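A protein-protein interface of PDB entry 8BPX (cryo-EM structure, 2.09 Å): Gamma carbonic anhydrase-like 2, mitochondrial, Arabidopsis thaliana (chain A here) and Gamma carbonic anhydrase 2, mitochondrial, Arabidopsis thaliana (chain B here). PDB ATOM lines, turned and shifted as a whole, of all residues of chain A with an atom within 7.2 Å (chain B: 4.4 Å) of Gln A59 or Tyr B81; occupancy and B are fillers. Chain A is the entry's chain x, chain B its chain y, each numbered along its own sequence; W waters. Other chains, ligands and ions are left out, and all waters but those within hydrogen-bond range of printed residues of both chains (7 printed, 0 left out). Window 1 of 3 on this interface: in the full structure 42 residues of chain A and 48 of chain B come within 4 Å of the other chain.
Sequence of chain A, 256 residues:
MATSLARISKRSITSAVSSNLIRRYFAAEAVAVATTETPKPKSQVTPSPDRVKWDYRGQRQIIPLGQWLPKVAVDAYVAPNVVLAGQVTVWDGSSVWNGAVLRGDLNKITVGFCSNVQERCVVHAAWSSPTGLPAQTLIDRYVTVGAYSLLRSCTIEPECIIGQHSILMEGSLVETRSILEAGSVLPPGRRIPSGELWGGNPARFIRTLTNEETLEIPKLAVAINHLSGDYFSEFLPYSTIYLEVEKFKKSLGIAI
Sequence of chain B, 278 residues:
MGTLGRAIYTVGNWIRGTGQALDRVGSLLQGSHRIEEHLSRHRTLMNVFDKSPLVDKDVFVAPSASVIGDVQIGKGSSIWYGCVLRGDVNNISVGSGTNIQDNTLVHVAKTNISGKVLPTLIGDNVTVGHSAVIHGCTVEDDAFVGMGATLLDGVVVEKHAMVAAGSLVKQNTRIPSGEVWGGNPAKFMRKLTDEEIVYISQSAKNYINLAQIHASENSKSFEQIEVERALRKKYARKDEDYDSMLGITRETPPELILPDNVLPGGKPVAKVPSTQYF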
ATOM      1  N   ASP A  55      12.183   8.332  -3.579  1.00  0.00           N
ATOM      2  CA  ASP A  55      13.594   8.497  -3.248  1.00  0.00           C
ATOM      3  C   ASP A  55      13.937   9.974  -3.416  1.00  0.00           C
ATOM      4  O   ASP A  55      13.907  10.500  -4.533  1.00  0.00           O
ATOM      5  CB  ASP A  55      14.458   7.609  -4.143  1.00  0.00           C
ATOM      6  CG  ASP A  55      15.914   7.556  -3.706  1.00  0.00           C
ATOM      7  OD1 ASP A  55      16.433   8.556  -3.174  1.00  0.00           O
ATOM      8  OD2 ASP A  55      16.552   6.506  -3.917  1.00  0.00           O
ATOM      9  N   TYR A  56      14.272  10.639  -2.305  1.00  0.00           N
ATOM     10  CA  TYR A  56      14.523  12.077  -2.339  1.00  0.00           C
ATOM     11  C   TYR A  56      15.703  12.442  -3.227  1.00  0.00           C
ATOM     12  O   TYR A  56      15.788  13.585  -3.684  1.00  0.00           O
ATOM     13  CB  TYR A  56      14.756  12.616  -0.922  1.00  0.00           C
ATOM     14  CG  TYR A  56      16.090  12.243  -0.306  1.00  0.00           C
ATOM     15  CD1 TYR A  56      16.244  11.054   0.386  1.00  0.00           C
ATOM     16  CD2 TYR A  56      17.193  13.086  -0.407  1.00  0.00           C
ATOM     17  CE1 TYR A  56      17.451  10.706   0.955  1.00  0.00           C
ATOM     18  CE2 TYR A  56      18.411  12.746   0.163  1.00  0.00           C
ATOM     19  CZ  TYR A  56      18.531  11.552   0.842  1.00  0.00           C
ATOM     20  OH  TYR A  56      19.730  11.192   1.414  1.00  0.00           O
ATOM     21  N   ARG A  57      16.611  11.503  -3.481  1.00  0.00           N
ATOM     22  CA  ARG A  57      17.793  11.799  -4.276  1.00  0.00           C
ATOM     23  C   ARG A  57      17.520  11.782  -5.773  1.00  0.00           C
ATOM     24  O   ARG A  57      18.331  12.307  -6.541  1.00  0.00           O
ATOM     25  CB  ARG A  57      18.906  10.804  -3.945  1.00  0.00           C
ATOM     26  CG  ARG A  57      19.083  10.558  -2.456  1.00  0.00           C
ATOM     27  CD  ARG A  57      19.892   9.306  -2.185  1.00  0.00           C
ATOM     28  NE  ARG A  57      19.141   8.077  -2.414  1.00  0.00           N
ATOM     29  CZ  ARG A  57      19.642   6.858  -2.252  1.00  0.00           C
ATOM     30  NH1 ARG A  57      20.886   6.672  -1.842  1.00  0.00           N
ATOM     31  NH2 ARG A  57      18.878   5.802  -2.512  1.00  0.00           N
ATOM     32  N   GLY A  58      16.398  11.213  -6.201  1.00  0.00           N
ATOM     33  CA  GLY A  58      16.159  10.998  -7.612  1.00  0.00           C
ATOM     34  C   GLY A  58      17.042   9.878  -8.141  1.00  0.00           C
ATOM     35  O   GLY A  58      17.782   9.226  -7.412  1.00  0.00           O
ATOM     36  N   GLN A  59      16.957   9.665  -9.448  1.00  0.00           N
ATOM     37  CA  GLN A  59      17.761   8.639 -10.097  1.00  0.00           C
ATOM     38  C   GLN A  59      19.199   9.125 -10.225  1.00  0.00           C
ATOM     39  O   GLN A  59      19.447  10.192 -10.793  1.00  0.00           O
ATOM     40  CB  GLN A  59      17.180   8.300 -11.468  1.00  0.00           C
ATOM     41  CG  GLN A  59      18.104   7.470 -12.340  1.00  0.00           C
ATOM     42  CD  GLN A  59      18.250   6.042 -11.842  1.00  0.00           C
ATOM     43  OE1 GLN A  59      17.272   5.306 -11.754  1.00  0.00           O
ATOM     44  NE2 GLN A  59      19.473   5.649 -11.517  1.00  0.00           N
ATOM     45  N   ARG A  60      20.144   8.348  -9.699  1.00  0.00           N
ATOM     46  CA  ARG A  60      21.554   8.674  -9.875  1.00  0.00           C
ATOM     47  C   ARG A  60      21.930   8.620 -11.350  1.00  0.00           C
ATOM     48  O   ARG A  60      21.572   7.677 -12.062  1.00  0.00           O
ATOM     49  CB  ARG A  60      22.434   7.716  -9.075  1.00  0.00           C
ATOM     50  CG  ARG A  60      23.094   8.350  -7.864  1.00  0.00           C
ATOM     51  CD  ARG A  60      24.176   7.462  -7.271  1.00  0.00           C
ATOM     52  NE  ARG A  60      23.648   6.192  -6.790  1.00  0.00           N
ATOM     53  CZ  ARG A  60      24.342   5.064  -6.746  1.00  0.00           C
ATOM     54  NH1 ARG A  60      25.602   5.013  -7.145  1.00  0.00           N
ATOM     55  NH2 ARG A  60      23.758   3.961  -6.290  1.00  0.00           N
ATOM     56  N   GLN A  61      22.659   9.639 -11.806  1.00  0.00           N
ATOM     57  CA  GLN A  61      23.074   9.688 -13.203  1.00  0.00           C
ATOM     58  C   GLN A  61      24.141   8.642 -13.509  1.00  0.00           C
ATOM     59  O   GLN A  61      24.117   8.018 -14.577  1.00  0.00           O
ATOM     60  CB  GLN A  61      23.581  11.087 -13.551  1.00  0.00           C
ATOM     61  CG  GLN A  61      24.013  11.245 -14.994  1.00  0.00           C
ATOM     62  CD  GLN A  61      24.532  12.635 -15.306  1.00  0.00           C
ATOM     63  OE1 GLN A  61      25.683  12.955 -15.027  1.00  0.00           O
ATOM     64  NE2 GLN A  61      23.682  13.465 -15.894  1.00  0.00           N
ATOM     65  N   ILE A  62      25.084   8.442 -12.595  1.00  0.00           N
ATOM     66  CA  ILE A  62      26.215   7.545 -12.802  1.00  0.00           C
ATOM     67  C   ILE A  62      25.961   6.287 -11.983  1.00  0.00           C
ATOM     68  O   ILE A  62      25.960   6.327 -10.748  1.00  0.00           O
ATOM     69  CB  ILE A  62      27.545   8.201 -12.406  1.00  0.00           C
ATOM     70  CG1 ILE A  62      27.798   9.459 -13.243  1.00  0.00           C
ATOM     71  CG2 ILE A  62      28.693   7.207 -12.543  1.00  0.00           C
ATOM     72  CD1 ILE A  62      27.936   9.193 -14.710  1.00  0.00           C
ATOM     73  N   ILE A  63      25.760   5.167 -12.666  1.00  0.00           N
ATOM     74  CA  ILE A  63      25.518   3.896 -11.993  1.00  0.00           C
ATOM     75  C   ILE A  63      26.753   3.017 -12.155  1.00  0.00           C
ATOM     76  O   ILE A  63      26.977   2.456 -13.235  1.00  0.00           O
ATOM     77  CB  ILE A  63      24.262   3.201 -12.545  1.00  0.00           C
ATOM     78  CG1 ILE A  63      23.014   4.045 -12.264  1.00  0.00           C
ATOM     79  CG2 ILE A  63      24.118   1.801 -11.958  1.00  0.00           C
ATOM     80  CD1 ILE A  63      22.692   4.192 -10.798  1.00  0.00           C
ATOM     81  N   LEU A  65      28.950  -0.428 -11.617  1.00  0.00           N
ATOM     82  CA  LEU A  65      28.590  -1.848 -11.604  1.00  0.00           C
ATOM     83  C   LEU A  65      29.864  -2.619 -11.264  1.00  0.00           C
ATOM     84  O   LEU A  65      30.652  -2.956 -12.148  1.00  0.00           O
ATOM     85  CB  LEU A  65      27.997  -2.276 -12.941  1.00  0.00           C
ATOM     86  CG  LEU A  65      26.578  -1.786 -13.260  1.00  0.00           C
ATOM     87  CD1 LEU A  65      26.093  -2.352 -14.582  1.00  0.00           C
ATOM     88  CD2 LEU A  65      25.607  -2.133 -12.146  1.00  0.00           C
ATOM     89  N   PRO A  80      21.116  16.139 -17.180  1.00  0.00           N
ATOM     90  CA  PRO A  80      20.969  15.683 -15.784  1.00  0.00           C
ATOM     91  C   PRO A  80      20.204  14.379 -15.617  1.00  0.00           C
ATOM     92  O   PRO A  80      20.546  13.592 -14.728  1.00  0.00           O
ATOM     93  CB  PRO A  80      20.237  16.857 -15.117  1.00  0.00           C
ATOM     94  CG  PRO A  80      20.567  18.033 -15.960  1.00  0.00           C
ATOM     95  CD  PRO A  80      20.628  17.517 -17.363  1.00  0.00           C
ATOM     96  N   ASN A  81      19.187  14.113 -16.436  1.00  0.00           N
ATOM     97  CA  ASN A  81      18.361  12.927 -16.243  1.00  0.00           C
ATOM     98  C   ASN A  81      18.819  11.733 -17.080  1.00  0.00           C
ATOM     99  O   ASN A  81      18.126  10.713 -17.109  1.00  0.00           O
ATOM    100  CB  ASN A  81      16.887  13.249 -16.524  1.00  0.00           C
ATOM    101  CG  ASN A  81      16.606  13.528 -17.987  1.00  0.00           C
ATOM    102  OD1 ASN A  81      17.498  13.883 -18.752  1.00  0.00           O
ATOM    103  ND2 ASN A  81      15.347  13.391 -18.375  1.00  0.00           N
ATOM    104  N   VAL A  82      19.967  11.839 -17.751  1.00  0.00           N
ATOM    105  CA  VAL A  82      20.553  10.697 -18.442  1.00  0.00           C
ATOM    106  C   VAL A  82      21.018   9.663 -17.419  1.00  0.00           C
ATOM    107  O   VAL A  82      21.441  10.002 -16.306  1.00  0.00           O
ATOM    108  CB  VAL A  82      21.720  11.166 -19.334  1.00  0.00           C
ATOM    109  CG1 VAL A  82      22.528   9.988 -19.869  1.00  0.00           C
ATOM    110  CG2 VAL A  82      21.208  12.029 -20.473  1.00  0.00           C
ATOM    111  N   VAL A  83      20.936   8.388 -17.788  1.00  0.00           N
ATOM    112  CA  VAL A  83      21.477   7.299 -16.980  1.00  0.00           C
ATOM    113  C   VAL A  83      22.634   6.666 -17.742  1.00  0.00           C
ATOM    114  O   VAL A  83      22.470   6.229 -18.886  1.00  0.00           O
ATOM    115  CB  VAL A  83      20.403   6.255 -16.641  1.00  0.00           C
ATOM    116  CG1 VAL A  83      21.037   5.044 -15.966  1.00  0.00           C
ATOM    117  CG2 VAL A  83      19.327   6.868 -15.756  1.00  0.00           C
ATOM    118  N   LEU A  84      23.805   6.630 -17.112  1.00  0.00           N
ATOM    119  CA  LEU A  84      24.969   5.910 -17.617  1.00  0.00           C
ATOM    120  C   LEU A  84      25.303   4.809 -16.621  1.00  0.00           C
ATOM    121  O   LEU A  84      25.525   5.089 -15.438  1.00  0.00           O
ATOM    122  CB  LEU A  84      26.168   6.841 -17.809  1.00  0.00           C
ATOM    123  CG  LEU A  84      25.985   8.157 -18.569  1.00  0.00           C
ATOM    124  CD1 LEU A  84      27.267   8.971 -18.525  1.00  0.00           C
ATOM    125  CD2 LEU A  84      25.552   7.915 -20.008  1.00  0.00           C
ATOM    126  N   ALA A  85      25.337   3.566 -17.089  1.00  0.00           N
ATOM    127  CA  ALA A  85      25.558   2.424 -16.210  1.00  0.00           C
ATOM    128  C   ALA A  85      26.663   1.534 -16.759  1.00  0.00           C
ATOM    129  O   ALA A  85      26.639   1.161 -17.934  1.00  0.00           O
ATOM    130  CB  ALA A  85      24.269   1.618 -16.023  1.00  0.00           C
ATOM    131  N   GLY A  99      16.816  12.251 -21.249  1.00  0.00           N
ATOM    132  CA  GLY A  99      16.073  11.012 -21.322  1.00  0.00           C
ATOM    133  C   GLY A  99      16.797   9.845 -21.956  1.00  0.00           C
ATOM    134  O   GLY A  99      16.198   8.774 -22.095  1.00  0.00           O
ATOM    135  N   ALA A 100      18.053  10.013 -22.349  1.00  0.00           N
ATOM    136  CA  ALA A 100      18.808   8.920 -22.937  1.00  0.00           C
ATOM    137  C   ALA A 100      19.288   7.950 -21.863  1.00  0.00           C
ATOM    138  O   ALA A 100      19.496   8.321 -20.707  1.00  0.00           O
ATOM    139  CB  ALA A 100      20.000   9.453 -23.729  1.00  0.00           C
ATOM    140  N   VAL A 101      19.460   6.693 -22.263  1.00  0.00           N
ATOM    141  CA  VAL A 101      19.929   5.634 -21.376  1.00  0.00           C
ATOM    142  C   VAL A 101      21.063   4.902 -22.078  1.00  0.00           C
ATOM    143  O   VAL A 101      20.888   4.408 -23.198  1.00  0.00           O
ATOM    144  CB  VAL A 101      18.804   4.654 -21.000  1.00  0.00           C
ATOM    145  CG1 VAL A 101      19.348   3.509 -20.144  1.00  0.00           C
ATOM    146  CG2 VAL A 101      17.678   5.382 -20.282  1.00  0.00           C
ATOM    147  N   LEU A 102      22.221   4.836 -21.426  1.00  0.00           N
ATOM    148  CA  LEU A 102      23.384   4.115 -21.936  1.00  0.00           C
ATOM    149  C   LEU A 102      23.755   3.051 -20.911  1.00  0.00           C
ATOM    150  O   LEU A 102      24.286   3.369 -19.844  1.00  0.00           O
ATOM    151  CB  LEU A 102      24.553   5.065 -22.194  1.00  0.00           C
ATOM    152  CG  LEU A 102      24.537   5.857 -23.507  1.00  0.00           C
ATOM    153  CD1 LEU A 102      23.497   6.963 -23.466  1.00  0.00           C
ATOM    154  CD2 LEU A 102      25.913   6.426 -23.793  1.00  0.00           C
ATOM    155  N   ARG A 103      23.477   1.792 -21.232  1.00  0.00           N
ATOM    156  CA  ARG A 103      23.628   0.692 -20.281  1.00  0.00           C
ATOM    157  C   ARG A 103      24.715  -0.256 -20.779  1.00  0.00           C
ATOM    158  O   ARG A 103      24.473  -1.081 -21.664  1.00  0.00           O
ATOM    159  CB  ARG A 103      22.301  -0.033 -20.082  1.00  0.00           C
ATOM    160  CG  ARG A 103      22.323  -1.061 -18.966  1.00  0.00           C
ATOM    161  CD  ARG A 103      20.992  -1.124 -18.233  1.00  0.00           C
ATOM    162  NE  ARG A 103      19.882  -1.427 -19.127  1.00  0.00           N
ATOM    163  CZ  ARG A 103      19.514  -2.652 -19.474  1.00  0.00           C
ATOM    164  NH1 ARG A 103      20.155  -3.719 -19.026  1.00  0.00           N
ATOM    165  NH2 ARG A 103      18.479  -2.812 -20.293  1.00  0.00           N
ATOM    166  N   ASP A 105      26.152  -2.987 -19.307  1.00  0.00           N
ATOM    167  CA  ASP A 105      26.276  -4.104 -18.375  1.00  0.00           C
ATOM    168  C   ASP A 105      26.624  -5.425 -19.050  1.00  0.00           C
ATOM    169  O   ASP A 105      27.009  -6.369 -18.357  1.00  0.00           O
ATOM    170  CB  ASP A 105      24.991  -4.279 -17.550  1.00  0.00           C
ATOM    171  CG  ASP A 105      23.729  -4.146 -18.379  1.00  0.00           C
ATOM    172  OD1 ASP A 105      23.797  -4.257 -19.619  1.00  0.00           O
ATOM    173  OD2 ASP A 105      22.656  -3.940 -17.777  1.00  0.00           O
ATOM    174  N   ARG A 120      16.158  10.715 -25.552  1.00  0.00           N
ATOM    175  CA  ARG A 120      15.375   9.439 -25.457  1.00  0.00           C
ATOM    176  C   ARG A 120      15.986   8.298 -26.280  1.00  0.00           C
ATOM    177  O   ARG A 120      15.307   7.372 -26.570  1.00  0.00           O
ATOM    178  CB  ARG A 120      13.889   9.704 -25.717  1.00  0.00           C
ATOM    179  CG  ARG A 120      13.274  10.651 -24.693  1.00  0.00           C
ATOM    180  CD  ARG A 120      11.845  10.393 -24.282  1.00  0.00           C
ATOM    181  NE  ARG A 120      11.529   9.012 -23.977  1.00  0.00           N
ATOM    182  CZ  ARG A 120      11.518   8.464 -22.767  1.00  0.00           C
ATOM    183  NH1 ARG A 120      11.780   9.177 -21.685  1.00  0.00           N
ATOM    184  NH2 ARG A 120      11.216   7.187 -22.648  1.00  0.00           N
ATOM    185  N   VAL A 122      18.214   4.997 -26.580  1.00  0.00           N
ATOM    186  CA  VAL A 122      18.662   3.902 -25.728  1.00  0.00           C
ATOM    187  C   VAL A 122      19.826   3.219 -26.428  1.00  0.00           C
ATOM    188  O   VAL A 122      19.699   2.790 -27.581  1.00  0.00           O
ATOM    189  CB  VAL A 122      17.538   2.902 -25.416  1.00  0.00           C
ATOM    190  CG1 VAL A 122      18.043   1.807 -24.487  1.00  0.00           C
ATOM    191  CG2 VAL A 122      16.349   3.614 -24.790  1.00  0.00           C
ATOM    192  N   PHE B  60      13.177  -5.642  -9.281  1.00  0.00           N
ATOM    193  CA  PHE B  60      13.937  -4.428  -9.543  1.00  0.00           C
ATOM    194  C   PHE B  60      13.009  -3.406 -10.176  1.00  0.00           C
ATOM    195  O   PHE B  60      12.464  -3.639 -11.258  1.00  0.00           O
ATOM    196  CB  PHE B  60      15.136  -4.685 -10.456  1.00  0.00           C
ATOM    197  CG  PHE B  60      15.861  -3.422 -10.864  1.00  0.00           C
ATOM    198  CD1 PHE B  60      16.212  -2.475  -9.915  1.00  0.00           C
ATOM    199  CD2 PHE B  60      16.172  -3.176 -12.193  1.00  0.00           C
ATOM    200  CE1 PHE B  60      16.875  -1.315 -10.278  1.00  0.00           C
ATOM    201  CE2 PHE B  60      16.832  -2.014 -12.564  1.00  0.00           C
ATOM    202  CZ  PHE B  60      17.185  -1.082 -11.608  1.00  0.00           C
ATOM    203  N   ALA B  62      13.652   0.388 -11.237  1.00  0.00           N
ATOM    204  CA  ALA B  62      14.608   1.478 -11.315  1.00  0.00           C
ATOM    205  C   ALA B  62      13.992   2.733 -10.703  1.00  0.00           C
ATOM    206  O   ALA B  62      12.800   2.993 -10.894  1.00  0.00           O
ATOM    207  CB  ALA B  62      15.016   1.737 -12.766  1.00  0.00           C
ATOM    208  N   PRO B  63      14.763   3.513  -9.945  1.00  0.00           N
ATOM    209  CA  PRO B  63      14.202   4.728  -9.331  1.00  0.00           C
ATOM    210  C   PRO B  63      13.567   5.679 -10.333  1.00  0.00           C
ATOM    211  O   PRO B  63      12.580   6.344 -10.001  1.00  0.00           O
ATOM    212  CB  PRO B  63      15.418   5.365  -8.645  1.00  0.00           C
ATOM    213  CG  PRO B  63      16.364   4.233  -8.412  1.00  0.00           C
ATOM    214  CD  PRO B  63      16.155   3.262  -9.535  1.00  0.00           C
ATOM    215  N   SER B  64      14.096   5.755 -11.552  1.00  0.00           N
ATOM    216  CA  SER B  64      13.540   6.633 -12.576  1.00  0.00           C
ATOM    217  C   SER B  64      12.303   6.059 -13.255  1.00  0.00           C
ATOM    218  O   SER B  64      11.688   6.756 -14.067  1.00  0.00           O
ATOM    219  CB  SER B  64      14.599   6.945 -13.633  1.00  0.00           C
ATOM    220  OG  SER B  64      15.137   5.759 -14.183  1.00  0.00           O
ATOM    221  N   TRP B  80      12.861  -1.238 -15.824  1.00  0.00           N
ATOM    222  CA  TRP B  80      14.158  -0.615 -16.026  1.00  0.00           C
ATOM    223  C   TRP B  80      14.025   0.906 -16.135  1.00  0.00           C
ATOM    224  O   TRP B  80      12.952   1.478 -15.946  1.00  0.00           O
ATOM    225  CB  TRP B  80      14.843  -1.252 -17.236  1.00  0.00           C
ATOM    226  CG  TRP B  80      15.309  -2.643 -16.898  1.00  0.00           C
ATOM    227  CD1 TRP B  80      14.561  -3.785 -16.913  1.00  0.00           C
ATOM    228  CD2 TRP B  80      16.607  -3.022 -16.430  1.00  0.00           C
ATOM    229  NE1 TRP B  80      15.320  -4.855 -16.514  1.00  0.00           N
ATOM    230  CE2 TRP B  80      16.580  -4.415 -16.207  1.00  0.00           C
ATOM    231  CE3 TRP B  80      17.793  -2.324 -16.192  1.00  0.00           C
ATOM    232  CZ2 TRP B  80      17.692  -5.120 -15.757  1.00  0.00           C
ATOM    233  CZ3 TRP B  80      18.898  -3.026 -15.746  1.00  0.00           C
ATOM    234  CH2 TRP B  80      18.839  -4.410 -15.534  1.00  0.00           C
ATOM    235  N   TYR B  81      15.154   1.565 -16.404  1.00  0.00           N
ATOM    236  CA  TYR B  81      15.237   3.019 -16.321  1.00  0.00           C
ATOM    237  C   TYR B  81      14.293   3.692 -17.314  1.00  0.00           C
ATOM    238  O   TYR B  81      14.265   3.345 -18.497  1.00  0.00           O
ATOM    239  CB  TYR B  81      16.678   3.467 -16.575  1.00  0.00           C
ATOM    240  CG  TYR B  81      17.673   2.821 -15.638  1.00  0.00           C
ATOM    241  CD1 TYR B  81      17.805   3.254 -14.326  1.00  0.00           C
ATOM    242  CD2 TYR B  81      18.451   1.750 -16.056  1.00  0.00           C
ATOM    243  CE1 TYR B  81      18.703   2.656 -13.466  1.00  0.00           C
ATOM    244  CE2 TYR B  81      19.348   1.145 -15.207  1.00  0.00           C
ATOM    245  CZ  TYR B  81      19.470   1.600 -13.911  1.00  0.00           C
ATOM    246  OH  TYR B  81      20.362   0.999 -13.064  1.00  0.00           O
ATOM    247  N   GLY B  82      13.519   4.656 -16.821  1.00  0.00           N
ATOM    248  CA  GLY B  82      12.644   5.445 -17.662  1.00  0.00           C
ATOM    249  C   GLY B  82      11.345   4.779 -18.061  1.00  0.00           C
ATOM    250  O   GLY B  82      10.565   5.387 -18.802  1.00  0.00           O
ATOM    251  N   CYS B  83      11.089   3.556 -17.608  1.00  0.00           N
ATOM    252  CA  CYS B  83       9.834   2.887 -17.920  1.00  0.00           C
ATOM    253  C   CYS B  83       8.658   3.594 -17.255  1.00  0.00           C
ATOM    254  O   CYS B  83       8.770   4.132 -16.152  1.00  0.00           O
ATOM    255  CB  CYS B  83       9.873   1.429 -17.465  1.00  0.00           C
ATOM    256  SG  CYS B  83      11.158   0.435 -18.222  1.00  0.00           S
ATOM    257  N   ASP B 102      14.351  -0.500 -20.872  1.00  0.00           N
ATOM    258  CA  ASP B 102      14.431   0.933 -20.608  1.00  0.00           C
ATOM    259  C   ASP B 102      13.530   1.737 -21.539  1.00  0.00           C
ATOM    260  O   ASP B 102      13.381   1.415 -22.721  1.00  0.00           O
ATOM    261  CB  ASP B 102      15.878   1.402 -20.768  1.00  0.00           C
ATOM    262  CG  ASP B 102      16.880   0.416 -20.193  1.00  0.00           C
ATOM    263  OD1 ASP B 102      17.105  -0.632 -20.833  1.00  0.00           O
ATOM    264  OD2 ASP B 102      17.451   0.688 -19.121  1.00  0.00           O
ATOM    265  N   ASN B 103      12.921   2.787 -20.988  1.00  0.00           N
ATOM    266  CA  ASN B 103      12.147   3.780 -21.733  1.00  0.00           C
ATOM    267  C   ASN B 103      10.899   3.188 -22.386  1.00  0.00           C
ATOM    268  O   ASN B 103      10.388   3.742 -23.359  1.00  0.00           O
ATOM    269  CB  ASN B 103      13.015   4.482 -22.788  1.00  0.00           C
ATOM    270  CG  ASN B 103      13.882   5.589 -22.200  1.00  0.00           C
ATOM    271  OD1 ASN B 103      13.896   5.807 -20.992  1.00  0.00           O
ATOM    272  ND2 ASN B 103      14.613   6.287 -23.059  1.00  0.00           N
ATOM    273  N   HIS B 214      21.711  -4.439 -10.711  1.00  0.00           N
ATOM    274  CA  HIS B 214      21.185  -3.074 -10.794  1.00  0.00           C
ATOM    275  C   HIS B 214      20.390  -2.696  -9.543  1.00  0.00           C
ATOM    276  O   HIS B 214      20.522  -1.576  -9.034  1.00  0.00           O
ATOM    277  CB  HIS B 214      20.343  -2.897 -12.055  1.00  0.00           C
ATOM    278  CG  HIS B 214      21.160  -2.730 -13.297  1.00  0.00           C
ATOM    279  ND1 HIS B 214      21.498  -1.495 -13.806  1.00  0.00           N
ATOM    280  CD2 HIS B 214      21.727  -3.644 -14.119  1.00  0.00           C
ATOM    281  CE1 HIS B 214      22.227  -1.655 -14.895  1.00  0.00           C
ATOM    282  NE2 HIS B 214      22.379  -2.950 -15.108  1.00  0.00           N
ATOM    283  N   ASN B 218      21.296   0.449  -7.052  1.00  0.00           N
ATOM    284  CA  ASN B 218      20.396   1.596  -6.943  1.00  0.00           C
ATOM    285  C   ASN B 218      19.843   1.790  -5.535  1.00  0.00           C
ATOM    286  O   ASN B 218      19.320   2.868  -5.235  1.00  0.00           O
ATOM    287  CB  ASN B 218      19.241   1.463  -7.937  1.00  0.00           C
ATOM    288  CG  ASN B 218      19.592   1.995  -9.316  1.00  0.00           C
ATOM    289  OD1 ASN B 218      19.487   3.190  -9.578  1.00  0.00           O
ATOM    290  ND2 ASN B 218      20.005   1.103 -10.206  1.00  0.00           N
HETATM  291  O   HOH W   1      13.977   8.352  -8.815  1.00  0.00           O
HETATM  292  O   HOH W   2      10.543   8.315 -18.548  1.00  0.00           O
HETATM  293  O   HOH W   3      13.142   6.018 -25.653  1.00  0.00           O
HETATM  294  O   HOH W   4      15.076   7.601 -19.253  1.00  0.00           O
HETATM  295  O   HOH W   5      21.504   4.458  -4.376  1.00  0.00           O
HETATM  296  O   HOH W   6      19.747   5.914  -8.249  1.00  0.00           O
HETATM  297  O   HOH W   7      10.507   6.013 -24.939  1.00  0.00           O
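The backbone carbonyl oxygen of Leu A84 sits at hydrogen-bond distance from the backbone NH of Ile A63, at 2.8 Å. The side-chain amide oxygen (OD1) of Asn A81 lies within hydrogen-bond range of the backbone NH (N) of Gly A99 (3.1 Å).
Gln A59 touches Pro B63. Tyr B81 touches Gln A59 (CD1 to OE1, 3.3 Å). Tyr B81 touches Ile A63 (OH to CG2, 3.997 Å). His B214 touches Leu A65 (NE2 to CD1, 3.8 Å). Val A101 touches Asp B102. Val A101 touches Asn B103. Trp B80 touches Arg A103. CD of Arg A103 touches CE1 of His B214, 3.6 Å away. CG2 of Val A122 touches ND2 of Asn B103, at 3.6 Å.
The side-chain amide oxygen (OE1) of Gln A59 sits at hydrogen-bond distance from the backbone NH (N) of Ser B64. OD1 of Asn B218 sits at hydrogen-bond distance from NE2 of Gln A59 (3.1 Å). The side-chain amide nitrogen (ND2) of Asn B103 lies within hydrogen-bond range of the backbone carbonyl oxygen (O) of Gly A99 (3.1 Å). NH2 of Arg A103 lies within salt-bridge range of OD1 of Asp B102 (2.6 Å). OD2 of Asp A105 lies within hydrogen-bond range of NE2 of His B214. NH2 of Arg A120 sits close to OD1 of Asn B103 (3.4 Å).
Of chain B, only Pro B63 (3.2 Å), Ser B64 (3.2 Å), Tyr B81 (3.3 Å) and Asn B218 (3.1 Å) come within 4 Å of Gln A59. Printed residues of chain B within 4 Å of Leu A65: His B214 (3.8 Å). Printed residues of chain B within 4 Å of Asp A105: His B214 (2.9 Å). Printed residues of chain A within 4 Å of Tyr B81: Gln A59 (3.3 Å) and Ile A63 (3.997 Å). Cys B83 touches none of the printed residues of chain A. The nearest residue of chain B that does not touch Gln A59 is Ala B62 (4.3 Å). The nearest printed residue of chain A that does not touch Tyr B81 is Val A83 (4.04 Å). The nearest printed residue of chain A that does not touch His B214 is Ala A85 (4.02 Å).
Water W3 bridges the backbone carbonyl oxygen (O) of Arg A120 (2.7 Å) and the side-chain amide nitrogen (ND2) of Asn B103 (3.0 Å). Water W5 lies within hydrogen-bond range of O of Asn B218 (2.8 Å), NH2 of Arg A60 (3.0 Å) and NH1 of Arg A57 (3.4 Å). Water W2 lies within hydrogen-bond range of O of Gly B82 (2.9 Å) and NH1 of Arg A120 (3.5 Å).
Of the 24 printed residues of chain A, 9 touch a printed residue of chain B. Hydrophobic or aromatic side chains of chain A that line the printed part of chain B: Ile A63, Leu A65, Val A101 and Val A122. Along chain A the printed residues that touch a printed residue of chain B span positions 59 to 122. Hydrophobic or aromatic side chains of chain B within 4 Å of the printed part of chain A: Pro B63, Trp B80, Tyr B81 and His B214. Among the printed residues, 16 pairs touch across the chains. Among the printed residues, Asp or Glu carboxylates within 4 Å of a Lys or Arg side-chain nitrogen of the other chain: Arg A103 with Asp B102 (2.6 Å).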
